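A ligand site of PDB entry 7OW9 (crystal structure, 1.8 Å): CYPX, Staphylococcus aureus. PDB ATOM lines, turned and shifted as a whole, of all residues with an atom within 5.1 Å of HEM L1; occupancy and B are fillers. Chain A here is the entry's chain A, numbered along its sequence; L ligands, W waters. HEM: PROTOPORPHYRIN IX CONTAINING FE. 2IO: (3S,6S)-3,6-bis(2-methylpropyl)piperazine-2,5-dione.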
ATOM      1  N   LEU A  52      14.131  16.497   6.382  1.00  0.00           N
ATOM      2  CA  LEU A  52      12.857  17.171   6.118  1.00  0.00           C
ATOM      3  C   LEU A  52      11.918  17.110   7.304  1.00  0.00           C
ATOM      4  O   LEU A  52      11.084  18.000   7.480  1.00  0.00           O
ATOM      5  CB  LEU A  52      12.190  16.541   4.899  1.00  0.00           C
ATOM      6  CG  LEU A  52      12.970  16.606   3.578  1.00  0.00           C
ATOM      7  CD1 LEU A  52      12.233  15.843   2.489  1.00  0.00           C
ATOM      8  CD2 LEU A  52      13.190  18.055   3.160  1.00  0.00           C
ATOM      9  N   LEU A  63      15.944  29.376   0.828  1.00  0.00           N
ATOM     10  CA  LEU A  63      14.984  29.856  -0.157  1.00  0.00           C
ATOM     11  C   LEU A  63      14.992  31.371  -0.271  1.00  0.00           C
ATOM     12  O   LEU A  63      14.661  31.909  -1.343  1.00  0.00           O
ATOM     13  CB  LEU A  63      13.588  29.350   0.217  1.00  0.00           C
ATOM     14  CG  LEU A  63      13.371  27.879  -0.102  1.00  0.00           C
ATOM     15  CD1 LEU A  63      12.015  27.391   0.409  1.00  0.00           C
ATOM     16  CD2 LEU A  63      13.486  27.600  -1.591  1.00  0.00           C
ATOM     17  N   LEU A  76       5.747  30.554   0.915  1.00  0.00           N
ATOM     18  CA  LEU A  76       5.176  29.808   2.037  1.00  0.00           C
ATOM     19  C   LEU A  76       6.242  28.971   2.728  1.00  0.00           C
ATOM     20  O   LEU A  76       6.279  28.900   3.960  1.00  0.00           O
ATOM     21  CB  LEU A  76       4.018  28.918   1.572  1.00  0.00           C
ATOM     22  CG  LEU A  76       3.365  28.038   2.643  1.00  0.00           C
ATOM     23  CD1 LEU A  76       2.631  28.903   3.671  1.00  0.00           C
ATOM     24  CD2 LEU A  76       2.423  27.023   2.012  1.00  0.00           C
ATOM     25  N   ALA A  77       7.113  28.309   1.949  1.00  0.00           N
ATOM     26  CA  ALA A  77       8.098  27.418   2.548  1.00  0.00           C
ATOM     27  C   ALA A  77       9.112  28.159   3.406  1.00  0.00           C
ATOM     28  O   ALA A  77       9.800  27.521   4.216  1.00  0.00           O
ATOM     29  CB  ALA A  77       8.822  26.639   1.434  1.00  0.00           C
ATOM     30  N   HIS A  84       2.891  30.026   9.163  1.00  0.00           N
ATOM     31  CA  HIS A  84       2.962  29.031   8.108  1.00  0.00           C
ATOM     32  C   HIS A  84       1.752  28.112   8.126  1.00  0.00           C
ATOM     33  O   HIS A  84       1.147  27.829   7.089  1.00  0.00           O
ATOM     34  CB  HIS A  84       4.261  28.234   8.232  1.00  0.00           C
ATOM     35  CG  HIS A  84       4.243  26.947   7.464  1.00  0.00           C
ATOM     36  ND1 HIS A  84       3.877  25.739   8.038  1.00  0.00           N
ATOM     37  CD2 HIS A  84       4.481  26.691   6.158  1.00  0.00           C
ATOM     38  CE1 HIS A  84       3.944  24.787   7.115  1.00  0.00           C
ATOM     39  NE2 HIS A  84       4.297  25.341   5.970  1.00  0.00           N
ATOM     40  N   LYS A  88      -0.759  28.196   4.988  1.00  0.00           N
ATOM     41  CA  LYS A  88      -0.850  26.913   4.302  1.00  0.00           C
ATOM     42  C   LYS A  88      -2.303  26.447   4.251  1.00  0.00           C
ATOM     43  O   LYS A  88      -2.776  25.987   3.209  1.00  0.00           O
ATOM     44  CB  LYS A  88       0.016  25.872   5.020  1.00  0.00           C
ATOM     45  CG  LYS A  88      -0.035  24.476   4.407  1.00  0.00           C
ATOM     46  CD  LYS A  88       1.181  23.638   4.845  1.00  0.00           C
ATOM     47  CE  LYS A  88       1.347  22.370   3.997  1.00  0.00           C
ATOM     48  NZ  LYS A  88       2.573  21.612   4.357  1.00  0.00           N
ATOM     49  N   ILE A  91      -4.153  28.396   1.607  1.00  0.00           N
ATOM     50  CA  ILE A  91      -3.891  27.943   0.250  1.00  0.00           C
ATOM     51  C   ILE A  91      -4.626  26.645  -0.016  1.00  0.00           C
ATOM     52  O   ILE A  91      -5.179  26.440  -1.098  1.00  0.00           O
ATOM     53  CB  ILE A  91      -2.366  27.809   0.039  1.00  0.00           C
ATOM     54  CG1 ILE A  91      -1.747  29.201  -0.035  1.00  0.00           C
ATOM     55  CG2 ILE A  91      -2.072  27.041  -1.227  1.00  0.00           C
ATOM     56  CD1 ILE A  91      -0.248  29.220   0.031  1.00  0.00           C
ATOM     57  N   MET A  95      -8.039  24.746  -3.005  1.00  0.00           N
ATOM     58  CA  MET A  95      -8.059  23.525  -3.805  1.00  0.00           C
ATOM     59  C   MET A  95      -8.757  22.398  -3.062  1.00  0.00           C
ATOM     60  O   MET A  95      -8.516  21.214  -3.324  1.00  0.00           O
ATOM     61  CB  MET A  95      -6.639  23.144  -4.261  1.00  0.00           C
ATOM     62  CG  MET A  95      -5.691  22.498  -3.262  1.00  0.00           C
ATOM     63  SD  MET A  95      -3.975  22.884  -3.744  1.00  0.00           S
ATOM     64  CE  MET A  95      -3.560  24.235  -2.631  1.00  0.00           C
ATOM     65  N   LEU A 142      -6.792  27.888 -10.894  1.00  0.00           N
ATOM     66  CA  LEU A 142      -6.771  27.800  -9.438  1.00  0.00           C
ATOM     67  C   LEU A 142      -6.643  29.182  -8.814  1.00  0.00           C
ATOM     68  O   LEU A 142      -7.376  29.517  -7.870  1.00  0.00           O
ATOM     69  CB  LEU A 142      -5.612  26.893  -9.005  1.00  0.00           C
ATOM     70  CG  LEU A 142      -5.197  26.865  -7.541  1.00  0.00           C
ATOM     71  CD1 LEU A 142      -6.346  26.245  -6.753  1.00  0.00           C
ATOM     72  CD2 LEU A 142      -3.938  26.036  -7.386  1.00  0.00           C
ATOM     73  N   ASN A 228       4.185  31.885  -5.956  1.00  0.00           N
ATOM     74  CA  ASN A 228       4.551  30.584  -5.371  1.00  0.00           C
ATOM     75  C   ASN A 228       3.628  29.488  -5.877  1.00  0.00           C
ATOM     76  O   ASN A 228       4.093  28.408  -6.278  1.00  0.00           O
ATOM     77  CB  ASN A 228       4.504  30.696  -3.837  1.00  0.00           C
ATOM     78  CG  ASN A 228       4.925  29.415  -3.100  1.00  0.00           C
ATOM     79  OD1 ASN A 228       4.946  29.393  -1.869  1.00  0.00           O
ATOM     80  ND2 ASN A 228       5.237  28.352  -3.838  1.00  0.00           N
ATOM     81  N   VAL A 229       2.325  29.742  -5.881  1.00  0.00           N
ATOM     82  CA  VAL A 229       1.386  28.744  -6.373  1.00  0.00           C
ATOM     83  C   VAL A 229       1.554  28.543  -7.877  1.00  0.00           C
ATOM     84  O   VAL A 229       1.547  27.407  -8.359  1.00  0.00           O
ATOM     85  CB  VAL A 229      -0.067  29.157  -6.015  1.00  0.00           C
ATOM     86  CG1 VAL A 229      -1.064  28.303  -6.781  1.00  0.00           C
ATOM     87  CG2 VAL A 229      -0.283  29.066  -4.510  1.00  0.00           C
ATOM     88  N   ALA A 232       4.800  26.492  -8.277  1.00  0.00           N
ATOM     89  CA  ALA A 232       4.765  25.158  -7.677  1.00  0.00           C
ATOM     90  C   ALA A 232       3.781  24.247  -8.384  1.00  0.00           C
ATOM     91  O   ALA A 232       4.020  23.036  -8.500  1.00  0.00           O
ATOM     92  CB  ALA A 232       4.419  25.275  -6.195  1.00  0.00           C
ATOM     93  N   ALA A 233       2.657  24.792  -8.845  1.00  0.00           N
ATOM     94  CA  ALA A 233       1.623  23.966  -9.471  1.00  0.00           C
ATOM     95  C   ALA A 233       1.916  23.668 -10.926  1.00  0.00           C
ATOM     96  O   ALA A 233       1.532  22.602 -11.425  1.00  0.00           O
ATOM     97  CB  ALA A 233       0.266  24.651  -9.346  1.00  0.00           C
ATOM     98  N   PRO A 236       5.789  20.903 -12.064  1.00  0.00           N
ATOM     99  CA  PRO A 236       5.848  19.433 -12.011  1.00  0.00           C
ATOM    100  C   PRO A 236       4.841  18.714 -12.906  1.00  0.00           C
ATOM    101  O   PRO A 236       4.959  17.493 -13.052  1.00  0.00           O
ATOM    102  CB  PRO A 236       5.553  19.119 -10.524  1.00  0.00           C
ATOM    103  CG  PRO A 236       5.798  20.453  -9.799  1.00  0.00           C
ATOM    104  CD  PRO A 236       5.253  21.446 -10.804  1.00  0.00           C
ATOM    105  N   THR A 240       5.292  15.029 -14.897  1.00  0.00           N
ATOM    106  CA  THR A 240       4.678  13.828 -14.331  1.00  0.00           C
ATOM    107  C   THR A 240       3.725  13.167 -15.314  1.00  0.00           C
ATOM    108  O   THR A 240       3.729  11.932 -15.454  1.00  0.00           O
ATOM    109  CB  THR A 240       3.969  14.187 -13.027  1.00  0.00           C
ATOM    110  OG1 THR A 240       4.900  14.822 -12.143  1.00  0.00           O
ATOM    111  CG2 THR A 240       3.399  12.941 -12.366  1.00  0.00           C
ATOM    112  N   LEU A 273       5.658   9.129  -9.674  1.00  0.00           N
ATOM    113  CA  LEU A 273       6.282  10.172  -8.859  1.00  0.00           C
ATOM    114  C   LEU A 273       7.481   9.620  -8.088  1.00  0.00           C
ATOM    115  O   LEU A 273       8.501  10.299  -7.948  1.00  0.00           O
ATOM    116  CB  LEU A 273       5.257  10.770  -7.893  1.00  0.00           C
ATOM    117  CG  LEU A 273       4.259  11.712  -8.596  1.00  0.00           C
ATOM    118  CD1 LEU A 273       3.057  12.001  -7.700  1.00  0.00           C
ATOM    119  CD2 LEU A 273       4.940  12.998  -9.054  1.00  0.00           C
ATOM    120  N   PRO A 278       9.672  14.374 -10.275  1.00  0.00           N
ATOM    121  CA  PRO A 278       9.832  15.600 -11.081  1.00  0.00           C
ATOM    122  C   PRO A 278      10.534  16.707 -10.327  1.00  0.00           C
ATOM    123  O   PRO A 278      11.234  17.516 -10.940  1.00  0.00           O
ATOM    124  CB  PRO A 278       8.383  15.969 -11.430  1.00  0.00           C
ATOM    125  CG  PRO A 278       7.580  15.412 -10.280  1.00  0.00           C
ATOM    126  CD  PRO A 278       8.267  14.117  -9.921  1.00  0.00           C
ATOM    127  N   VAL A 279      10.361  16.778  -9.013  1.00  0.00           N
ATOM    128  CA  VAL A 279      11.155  17.676  -8.173  1.00  0.00           C
ATOM    129  C   VAL A 279      12.252  16.816  -7.538  1.00  0.00           C
ATOM    130  O   VAL A 279      11.979  15.967  -6.686  1.00  0.00           O
ATOM    131  CB  VAL A 279      10.294  18.385  -7.126  1.00  0.00           C
ATOM    132  CG1 VAL A 279      11.154  19.329  -6.317  1.00  0.00           C
ATOM    133  CG2 VAL A 279       9.154  19.142  -7.812  1.00  0.00           C
ATOM    134  N   ILE A 282      15.715  19.243  -2.839  1.00  0.00           N
ATOM    135  CA  ILE A 282      15.146  20.146  -1.834  1.00  0.00           C
ATOM    136  C   ILE A 282      16.244  20.672  -0.930  1.00  0.00           C
ATOM    137  O   ILE A 282      16.784  19.908  -0.108  1.00  0.00           O
ATOM    138  CB  ILE A 282      14.071  19.450  -0.980  1.00  0.00           C
ATOM    139  CG1 ILE A 282      12.885  18.931  -1.801  1.00  0.00           C
ATOM    140  CG2 ILE A 282      13.550  20.392   0.094  1.00  0.00           C
ATOM    141  CD1 ILE A 282      11.833  18.186  -0.953  1.00  0.00           C
ATOM    142  N   PRO A 283      16.581  21.955  -0.993  1.00  0.00           N
ATOM    143  CA  PRO A 283      17.636  22.484  -0.122  1.00  0.00           C
ATOM    144  C   PRO A 283      17.135  22.901   1.251  1.00  0.00           C
ATOM    145  O   PRO A 283      15.965  23.268   1.445  1.00  0.00           O
ATOM    146  CB  PRO A 283      18.167  23.694  -0.902  1.00  0.00           C
ATOM    147  CG  PRO A 283      17.292  23.844  -2.145  1.00  0.00           C
ATOM    148  CD  PRO A 283      16.090  22.960  -1.951  1.00  0.00           C
ATOM    149  N   ARG A 284      18.056  22.845   2.215  1.00  0.00           N
ATOM    150  CA  ARG A 284      17.857  23.314   3.570  1.00  0.00           C
ATOM    151  C   ARG A 284      19.172  23.883   4.071  1.00  0.00           C
ATOM    152  O   ARG A 284      20.241  23.585   3.538  1.00  0.00           O
ATOM    153  CB  ARG A 284      17.412  22.178   4.509  1.00  0.00           C
ATOM    154  CG  ARG A 284      16.044  21.589   4.205  1.00  0.00           C
ATOM    155  CD  ARG A 284      14.930  22.562   4.564  1.00  0.00           C
ATOM    156  NE  ARG A 284      13.598  21.955   4.540  1.00  0.00           N
ATOM    157  CZ  ARG A 284      12.755  22.049   3.529  1.00  0.00           C
ATOM    158  NH1 ARG A 284      13.100  22.625   2.390  1.00  0.00           N
ATOM    159  NH2 ARG A 284      11.537  21.535   3.651  1.00  0.00           N
ATOM    160  N   LEU A 342       8.983  10.343  -1.184  1.00  0.00           N
ATOM    161  CA  LEU A 342       9.263  11.708  -0.736  1.00  0.00           C
ATOM    162  C   LEU A 342       9.060  12.733  -1.836  1.00  0.00           C
ATOM    163  O   LEU A 342       9.521  13.869  -1.731  1.00  0.00           O
ATOM    164  CB  LEU A 342      10.712  11.777  -0.228  1.00  0.00           C
ATOM    165  CG  LEU A 342      10.947  10.894   1.002  1.00  0.00           C
ATOM    166  CD1 LEU A 342      12.415  10.711   1.269  1.00  0.00           C
ATOM    167  CD2 LEU A 342      10.227  11.487   2.207  1.00  0.00           C
ATOM    168  N   SER A 343       8.357  12.344  -2.894  1.00  0.00           N
ATOM    169  CA  SER A 343       8.192  13.190  -4.077  1.00  0.00           C
ATOM    170  C   SER A 343       7.427  14.475  -3.800  1.00  0.00           C
ATOM    171  O   SER A 343       7.587  15.447  -4.536  1.00  0.00           O
ATOM    172  CB  SER A 343       7.530  12.359  -5.157  1.00  0.00           C
ATOM    173  OG  SER A 343       6.132  12.296  -4.958  1.00  0.00           O
ATOM    174  N   PHE A 344       6.619  14.505  -2.735  1.00  0.00           N
ATOM    175  CA  PHE A 344       5.973  15.723  -2.265  1.00  0.00           C
ATOM    176  C   PHE A 344       6.633  16.304  -1.025  1.00  0.00           C
ATOM    177  O   PHE A 344       6.060  17.175  -0.373  1.00  0.00           O
ATOM    178  CB  PHE A 344       4.484  15.454  -1.961  1.00  0.00           C
ATOM    179  CG  PHE A 344       3.633  15.158  -3.170  1.00  0.00           C
ATOM    180  CD1 PHE A 344       3.363  16.136  -4.106  1.00  0.00           C
ATOM    181  CD2 PHE A 344       3.067  13.909  -3.336  1.00  0.00           C
ATOM    182  CE1 PHE A 344       2.548  15.866  -5.198  1.00  0.00           C
ATOM    183  CE2 PHE A 344       2.263  13.627  -4.431  1.00  0.00           C
ATOM    184  CZ  PHE A 344       2.004  14.619  -5.354  1.00  0.00           C
ATOM    185  N   GLY A 345       7.821  15.821  -0.673  1.00  0.00           N
ATOM    186  CA  GLY A 345       8.447  16.208   0.586  1.00  0.00           C
ATOM    187  C   GLY A 345       7.810  15.465   1.754  1.00  0.00           C
ATOM    188  O   GLY A 345       7.055  14.505   1.606  1.00  0.00           O
ATOM    189  N   VAL A 348       6.947  19.520   7.904  1.00  0.00           N
ATOM    190  CA  VAL A 348       6.236  20.800   7.954  1.00  0.00           C
ATOM    191  C   VAL A 348       5.851  21.288   6.563  1.00  0.00           C
ATOM    192  O   VAL A 348       4.739  21.759   6.341  1.00  0.00           O
ATOM    193  CB  VAL A 348       7.108  21.833   8.688  1.00  0.00           C
ATOM    194  CG1 VAL A 348       6.487  23.217   8.617  1.00  0.00           C
ATOM    195  CG2 VAL A 348       7.313  21.416  10.150  1.00  0.00           C
ATOM    196  N   HIS A 349       6.762  21.183   5.597  1.00  0.00           N
ATOM    197  CA  HIS A 349       6.557  21.787   4.291  1.00  0.00           C
ATOM    198  C   HIS A 349       6.111  20.786   3.239  1.00  0.00           C
ATOM    199  O   HIS A 349       6.243  21.061   2.036  1.00  0.00           O
ATOM    200  CB  HIS A 349       7.837  22.498   3.864  1.00  0.00           C
ATOM    201  CG  HIS A 349       8.202  23.644   4.752  1.00  0.00           C
ATOM    202  ND1 HIS A 349       7.488  24.834   4.752  1.00  0.00           N
ATOM    203  CD2 HIS A 349       9.178  23.777   5.692  1.00  0.00           C
ATOM    204  CE1 HIS A 349       8.039  25.657   5.632  1.00  0.00           C
ATOM    205  NE2 HIS A 349       9.053  25.044   6.223  1.00  0.00           N
ATOM    206  N   THR A 350       5.542  19.659   3.647  1.00  0.00           N
ATOM    207  CA  THR A 350       4.946  18.730   2.699  1.00  0.00           C
ATOM    208  C   THR A 350       4.050  19.504   1.731  1.00  0.00           C
ATOM    209  O   THR A 350       3.303  20.399   2.141  1.00  0.00           O
ATOM    210  CB  THR A 350       4.120  17.669   3.420  1.00  0.00           C
ATOM    211  OG1 THR A 350       4.914  17.026   4.411  1.00  0.00           O
ATOM    212  CG2 THR A 350       3.622  16.617   2.429  1.00  0.00           C
ATOM    213  N   CYS A 351       4.140  19.171   0.452  1.00  0.00           N
ATOM    214  CA  CYS A 351       3.385  19.895  -0.584  1.00  0.00           C
ATOM    215  C   CYS A 351       1.916  20.054  -0.203  1.00  0.00           C
ATOM    216  O   CYS A 351       1.191  19.063  -0.030  1.00  0.00           O
ATOM    217  CB  CYS A 351       3.500  19.168  -1.916  1.00  0.00           C
ATOM    218  SG  CYS A 351       2.601  19.964  -3.265  1.00  0.00           S
ATOM    219  N   VAL A 352       1.466  21.297  -0.100  1.00  0.00           N
ATOM    220  CA  VAL A 352       0.056  21.554   0.198  1.00  0.00           C
ATOM    221  C   VAL A 352      -0.838  21.110  -0.957  1.00  0.00           C
ATOM    222  O   VAL A 352      -2.024  20.841  -0.747  1.00  0.00           O
ATOM    223  CB  VAL A 352      -0.136  23.037   0.537  1.00  0.00           C
ATOM    224  CG1 VAL A 352       0.170  23.909  -0.669  1.00  0.00           C
ATOM    225  CG2 VAL A 352      -1.532  23.301   1.092  1.00  0.00           C
ATOM    226  N   GLY A 353      -0.297  20.989  -2.174  1.00  0.00           N
ATOM    227  CA  GLY A 353      -1.057  20.576  -3.342  1.00  0.00           C
ATOM    228  C   GLY A 353      -0.947  19.112  -3.699  1.00  0.00           C
ATOM    229  O   GLY A 353      -1.318  18.748  -4.819  1.00  0.00           O
ATOM    230  N   PHE A 356      -4.522  17.526  -4.299  1.00  0.00           N
ATOM    231  CA  PHE A 356      -5.057  18.115  -5.511  1.00  0.00           C
ATOM    232  C   PHE A 356      -4.330  17.594  -6.737  1.00  0.00           C
ATOM    233  O   PHE A 356      -4.956  17.244  -7.752  1.00  0.00           O
ATOM    234  CB  PHE A 356      -4.975  19.642  -5.434  1.00  0.00           C
ATOM    235  CG  PHE A 356      -5.218  20.317  -6.753  1.00  0.00           C
ATOM    236  CD1 PHE A 356      -6.462  20.267  -7.360  1.00  0.00           C
ATOM    237  CD2 PHE A 356      -4.197  21.012  -7.397  1.00  0.00           C
ATOM    238  CE1 PHE A 356      -6.688  20.877  -8.570  1.00  0.00           C
ATOM    239  CE2 PHE A 356      -4.420  21.635  -8.618  1.00  0.00           C
ATOM    240  CZ  PHE A 356      -5.673  21.554  -9.190  1.00  0.00           C
ATOM    241  N   SER A 357      -2.998  17.495  -6.666  1.00  0.00           N
ATOM    242  CA  SER A 357      -2.217  17.013  -7.800  1.00  0.00           C
ATOM    243  C   SER A 357      -2.634  15.608  -8.208  1.00  0.00           C
ATOM    244  O   SER A 357      -2.761  15.318  -9.399  1.00  0.00           O
ATOM    245  CB  SER A 357      -0.720  17.009  -7.437  1.00  0.00           C
ATOM    246  OG  SER A 357      -0.203  18.312  -7.326  1.00  0.00           O
ATOM    247  N   LEU A 361      -4.209  14.861 -11.844  1.00  0.00           N
ATOM    248  CA  LEU A 361      -3.517  13.983 -12.768  1.00  0.00           C
ATOM    249  C   LEU A 361      -4.356  12.751 -13.106  1.00  0.00           C
ATOM    250  O   LEU A 361      -4.297  12.242 -14.227  1.00  0.00           O
ATOM    251  CB  LEU A 361      -2.169  13.553 -12.189  1.00  0.00           C
ATOM    252  CG  LEU A 361      -1.105  14.636 -12.082  1.00  0.00           C
ATOM    253  CD1 LEU A 361       0.060  14.224 -11.181  1.00  0.00           C
ATOM    254  CD2 LEU A 361      -0.581  15.033 -13.459  1.00  0.00           C
HETATM  255  CHA HEM L   1       5.902  22.152  -1.604  1.00  0.00           C
HETATM  256  CHB HEM L   1       6.419  18.853  -5.097  1.00  0.00           C
HETATM  257  CHC HEM L   1       2.209  20.322  -6.960  1.00  0.00           C
HETATM  258  CHD HEM L   1       2.140  24.101  -3.963  1.00  0.00           C
HETATM  259  C1A HEM L   1       6.380  21.100  -2.352  1.00  0.00           C
HETATM  260  C2A HEM L   1       7.540  20.294  -2.022  1.00  0.00           C
HETATM  261  C3A HEM L   1       7.669  19.375  -2.995  1.00  0.00           C
HETATM  262  C4A HEM L   1       6.616  19.583  -3.970  1.00  0.00           C
HETATM  263  CMA HEM L   1       8.745  18.281  -3.098  1.00  0.00           C
HETATM  264  CAA HEM L   1       8.426  20.458  -0.776  1.00  0.00           C
HETATM  265  CBA HEM L   1       9.399  21.626  -0.876  1.00  0.00           C
HETATM  266  CGA HEM L   1      10.230  21.779   0.383  1.00  0.00           C
HETATM  267  O1A HEM L   1      10.100  20.970   1.352  1.00  0.00           O
HETATM  268  O2A HEM L   1      11.043  22.729   0.414  1.00  0.00           O
HETATM  269  C1B HEM L   1       5.279  18.897  -5.872  1.00  0.00           C
HETATM  270  C2B HEM L   1       4.879  17.930  -6.871  1.00  0.00           C
HETATM  271  C3B HEM L   1       3.703  18.346  -7.392  1.00  0.00           C
HETATM  272  C4B HEM L   1       3.338  19.579  -6.725  1.00  0.00           C
HETATM  273  CMB HEM L   1       5.699  16.681  -7.236  1.00  0.00           C
HETATM  274  CAB HEM L   1       2.835  17.689  -8.492  1.00  0.00           C
HETATM  275  CBB HEM L   1       3.052  16.443  -8.903  1.00  0.00           C
HETATM  276  C1C HEM L   1       1.805  21.447  -6.294  1.00  0.00           C
HETATM  277  C2C HEM L   1       0.557  22.158  -6.529  1.00  0.00           C
HETATM  278  C3C HEM L   1       0.500  23.214  -5.728  1.00  0.00           C
HETATM  279  C4C HEM L   1       1.733  23.211  -4.924  1.00  0.00           C
HETATM  280  CMC HEM L   1      -0.495  21.733  -7.575  1.00  0.00           C
HETATM  281  CAC HEM L   1      -0.687  24.199  -5.693  1.00  0.00           C
HETATM  282  CBC HEM L   1      -0.664  25.280  -4.906  1.00  0.00           C
HETATM  283  C1D HEM L   1       3.156  23.885  -3.061  1.00  0.00           C
HETATM  284  C2D HEM L   1       3.459  24.726  -1.933  1.00  0.00           C
HETATM  285  C3D HEM L   1       4.499  24.206  -1.280  1.00  0.00           C
HETATM  286  C4D HEM L   1       4.877  22.990  -1.978  1.00  0.00           C
HETATM  287  CMD HEM L   1       2.702  26.018  -1.556  1.00  0.00           C
HETATM  288  CAD HEM L   1       5.152  24.764  -0.003  1.00  0.00           C
HETATM  289  CBD HEM L   1       4.504  24.007   1.152  1.00  0.00           C
HETATM  290  CGD HEM L   1       4.886  24.472   2.544  1.00  0.00           C
HETATM  291  O1D HEM L   1       5.870  25.230   2.675  1.00  0.00           O
HETATM  292  O2D HEM L   1       4.204  24.072   3.516  1.00  0.00           O
HETATM  293  NA  HEM L   1       5.843  20.642  -3.541  1.00  0.00           N
HETATM  294  NB  HEM L   1       4.319  19.882  -5.806  1.00  0.00           N
HETATM  295  NC  HEM L   1       2.485  22.133  -5.316  1.00  0.00           N
HETATM  296  ND  HEM L   1       4.040  22.823  -3.063  1.00  0.00           N
HETATM  297 FE   HEM L   1       4.072  21.252  -4.354  1.00  0.00          FE
HETATM  298  C1  2IO L   2      10.441  28.522  -3.854  1.00  0.00           C
HETATM  299  C10 2IO L   2      10.564  23.557  -6.948  1.00  0.00           C
HETATM  300  C11 2IO L   2       8.578  23.774  -8.450  1.00  0.00           C
HETATM  301  C12 2IO L   2       7.540  25.000  -3.261  1.00  0.00           C
HETATM  302  C2  2IO L   2       9.918  27.092  -4.005  1.00  0.00           C
HETATM  303  C3  2IO L   2       8.891  27.007  -5.106  1.00  0.00           C
HETATM  304  C4  2IO L   2       9.383  26.581  -2.672  1.00  0.00           C
HETATM  305  C5  2IO L   2       8.933  25.109  -2.665  1.00  0.00           C
HETATM  306  C6  2IO L   2       9.573  23.164  -4.077  1.00  0.00           C
HETATM  307  C7  2IO L   2       8.174  23.064  -4.663  1.00  0.00           C
HETATM  308  C8  2IO L   2       8.258  22.802  -6.174  1.00  0.00           C
HETATM  309  C9  2IO L   2       9.053  23.801  -7.007  1.00  0.00           C
HETATM  310  N1  2IO L   2       9.871  24.224  -3.328  1.00  0.00           N
HETATM  311  N2  2IO L   2       7.368  24.232  -4.330  1.00  0.00           N
HETATM  312  O1  2IO L   2      10.415  22.326  -4.378  1.00  0.00           O
HETATM  313  O2  2IO L   2       6.638  25.719  -2.818  1.00  0.00           O
HETATM  314  O   HOH W   1      12.281  23.903  -1.651  1.00  0.00           O
HETATM  315  O   HOH W   2       9.086  18.755   2.624  1.00  0.00           O
HETATM  316  O   HOH W   3       5.367  22.420  -5.842  1.00  0.00           O
HETATM  317  O   HOH W   4       6.656  27.728  -0.737  1.00  0.00           O
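The guanidinium group (NH2) of Arg 284 is in salt-bridge range of an oxygen (O1A) of HEM L1 (2.8 Å). The backbone NH (N) of Ala 77 sits close to an oxygen (O1D) of HEM L1, 3.4 Å away. An oxygen (O2) of 2IO L2 is in hydrogen-bond range of the side-chain amide nitrogen (ND2) of Asn 228, at 3.2 Å. The side-chain sulfur (SG) of Cys 351 binds an iron atom (FE) of HEM L1, 2.2 Å away. A ring nitrogen (NE2) of His 84 sits at hydrogen-bond distance from an oxygen (O2D) of HEM L1 (2.8 Å). An oxygen (O2D) of HEM L1 is in salt-bridge range of the side-chain amino group (NZ) of Lys 88, 3.1 Å away. O1D of HEM L1 lies within hydrogen-bond range of ND1 of His 349 (2.7 Å).
CD2 of Leu 76 touches CGD of HEM L1, at 3.6 Å. CE of Met 95 touches CBC of HEM L1 (3.8 Å). Val 229 touches HEM L1 (CG1 to CBC, 3.6 Å). Ala 232 touches HEM L1 (CB to CHD, 3.4 Å). CB of Ala 233 touches CMC of HEM L1 (3.5 Å). Pro 236 touches HEM L1 (CB to CAB, 3.7 Å). CD2 of Leu 273 touches CBB of HEM L1, 3.9 Å away. Pro 278 touches HEM L1. CG2 of Val 279 touches CHB of HEM L1 (3.9 Å). Ile 282 touches HEM L1 (CG2 to O2A, 3.4 Å). Ser 343 touches HEM L1 (O to CMA, 3.4 Å). CE1 of Phe 344 touches C3B of HEM L1, 3.5 Å away. Gly 345 touches HEM L1. Val 348 touches HEM L1 (O to O2D, 3.7 Å). O of Thr 350 touches CBD of HEM L1 (3.9 Å). CG1 of Val 352 touches CMD of HEM L1, 3.4 Å away. CA of Gly 353 touches C3C of HEM L1, at 3.9 Å. Phe 356 touches HEM L1. Ser 357 touches HEM L1 (OG to CHC, 3.2 Å). Hydrophobic or aromatic side chains that line HEM L1: Leu 76, Ala 77, His 84, Met 95, Val 229, Ala 232, Ala 233, Pro 236, Leu 273, Pro 278, Val 279, Ile 282, Phe 344, His 349, Val 352 and Phe 356. Within 4 Å of HEM L1: Leu 76, Ala 77, His 84, Lys 88, Met 95, Val 229, Ala 232, Ala 233, Pro 236, Leu 273, Pro 278, Val 279, Ile 282, Arg 284, Ser 343, Phe 344, Gly 345, Val 348, His 349, Thr 350, Cys 351, Val 352, Gly 353, Phe 356 and Ser 357. The nearest printed residue that does not touch HEM L1 is Asn 228 (4.1 Å).
Water W3 bridges O of Ala 232 (3.0 Å) and N2 of 2IO L2 (3.1 Å). Water W1 lies within hydrogen-bond range of an oxygen (O2A) of HEM L1 (2.7 Å) and a nitrogen (N1) of 2IO L2 (3.0 Å). Water W4 lies within hydrogen-bond range of OD1 of Asn 228, N of Ala 77, O2 of 2IO L2 and N of Leu 76.
ND1 of His 349 sits at hydrogen-bond distance from NE2 of His 84 (3.5 Å). The backbone carbonyl oxygen of Ala 77 sits close to a ring nitrogen (NE2) of His 349 (3.3 Å). O of Val 348 is in hydrogen-bond range of NZ of Lys 88. OG of Ser 357 sits at hydrogen-bond distance from O of Gly 353 (2.8 Å). The side-chain sulfur (SG) of Cys 351 sits close to the backbone NH (N) of Gly 353, at 3.3 Å. The backbone NH of Leu 76 is in hydrogen-bond range of the side-chain amide oxygen of Asn 228, 3.1 Å away. NZ of Lys 88 is in hydrogen-bond range of O of Thr 350, 2.6 Å away. The backbone carbonyl oxygen (O) of Pro 236 lies within hydrogen-bond range of the side-chain hydroxyl (OG1) of Thr 240 (2.8 Å).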
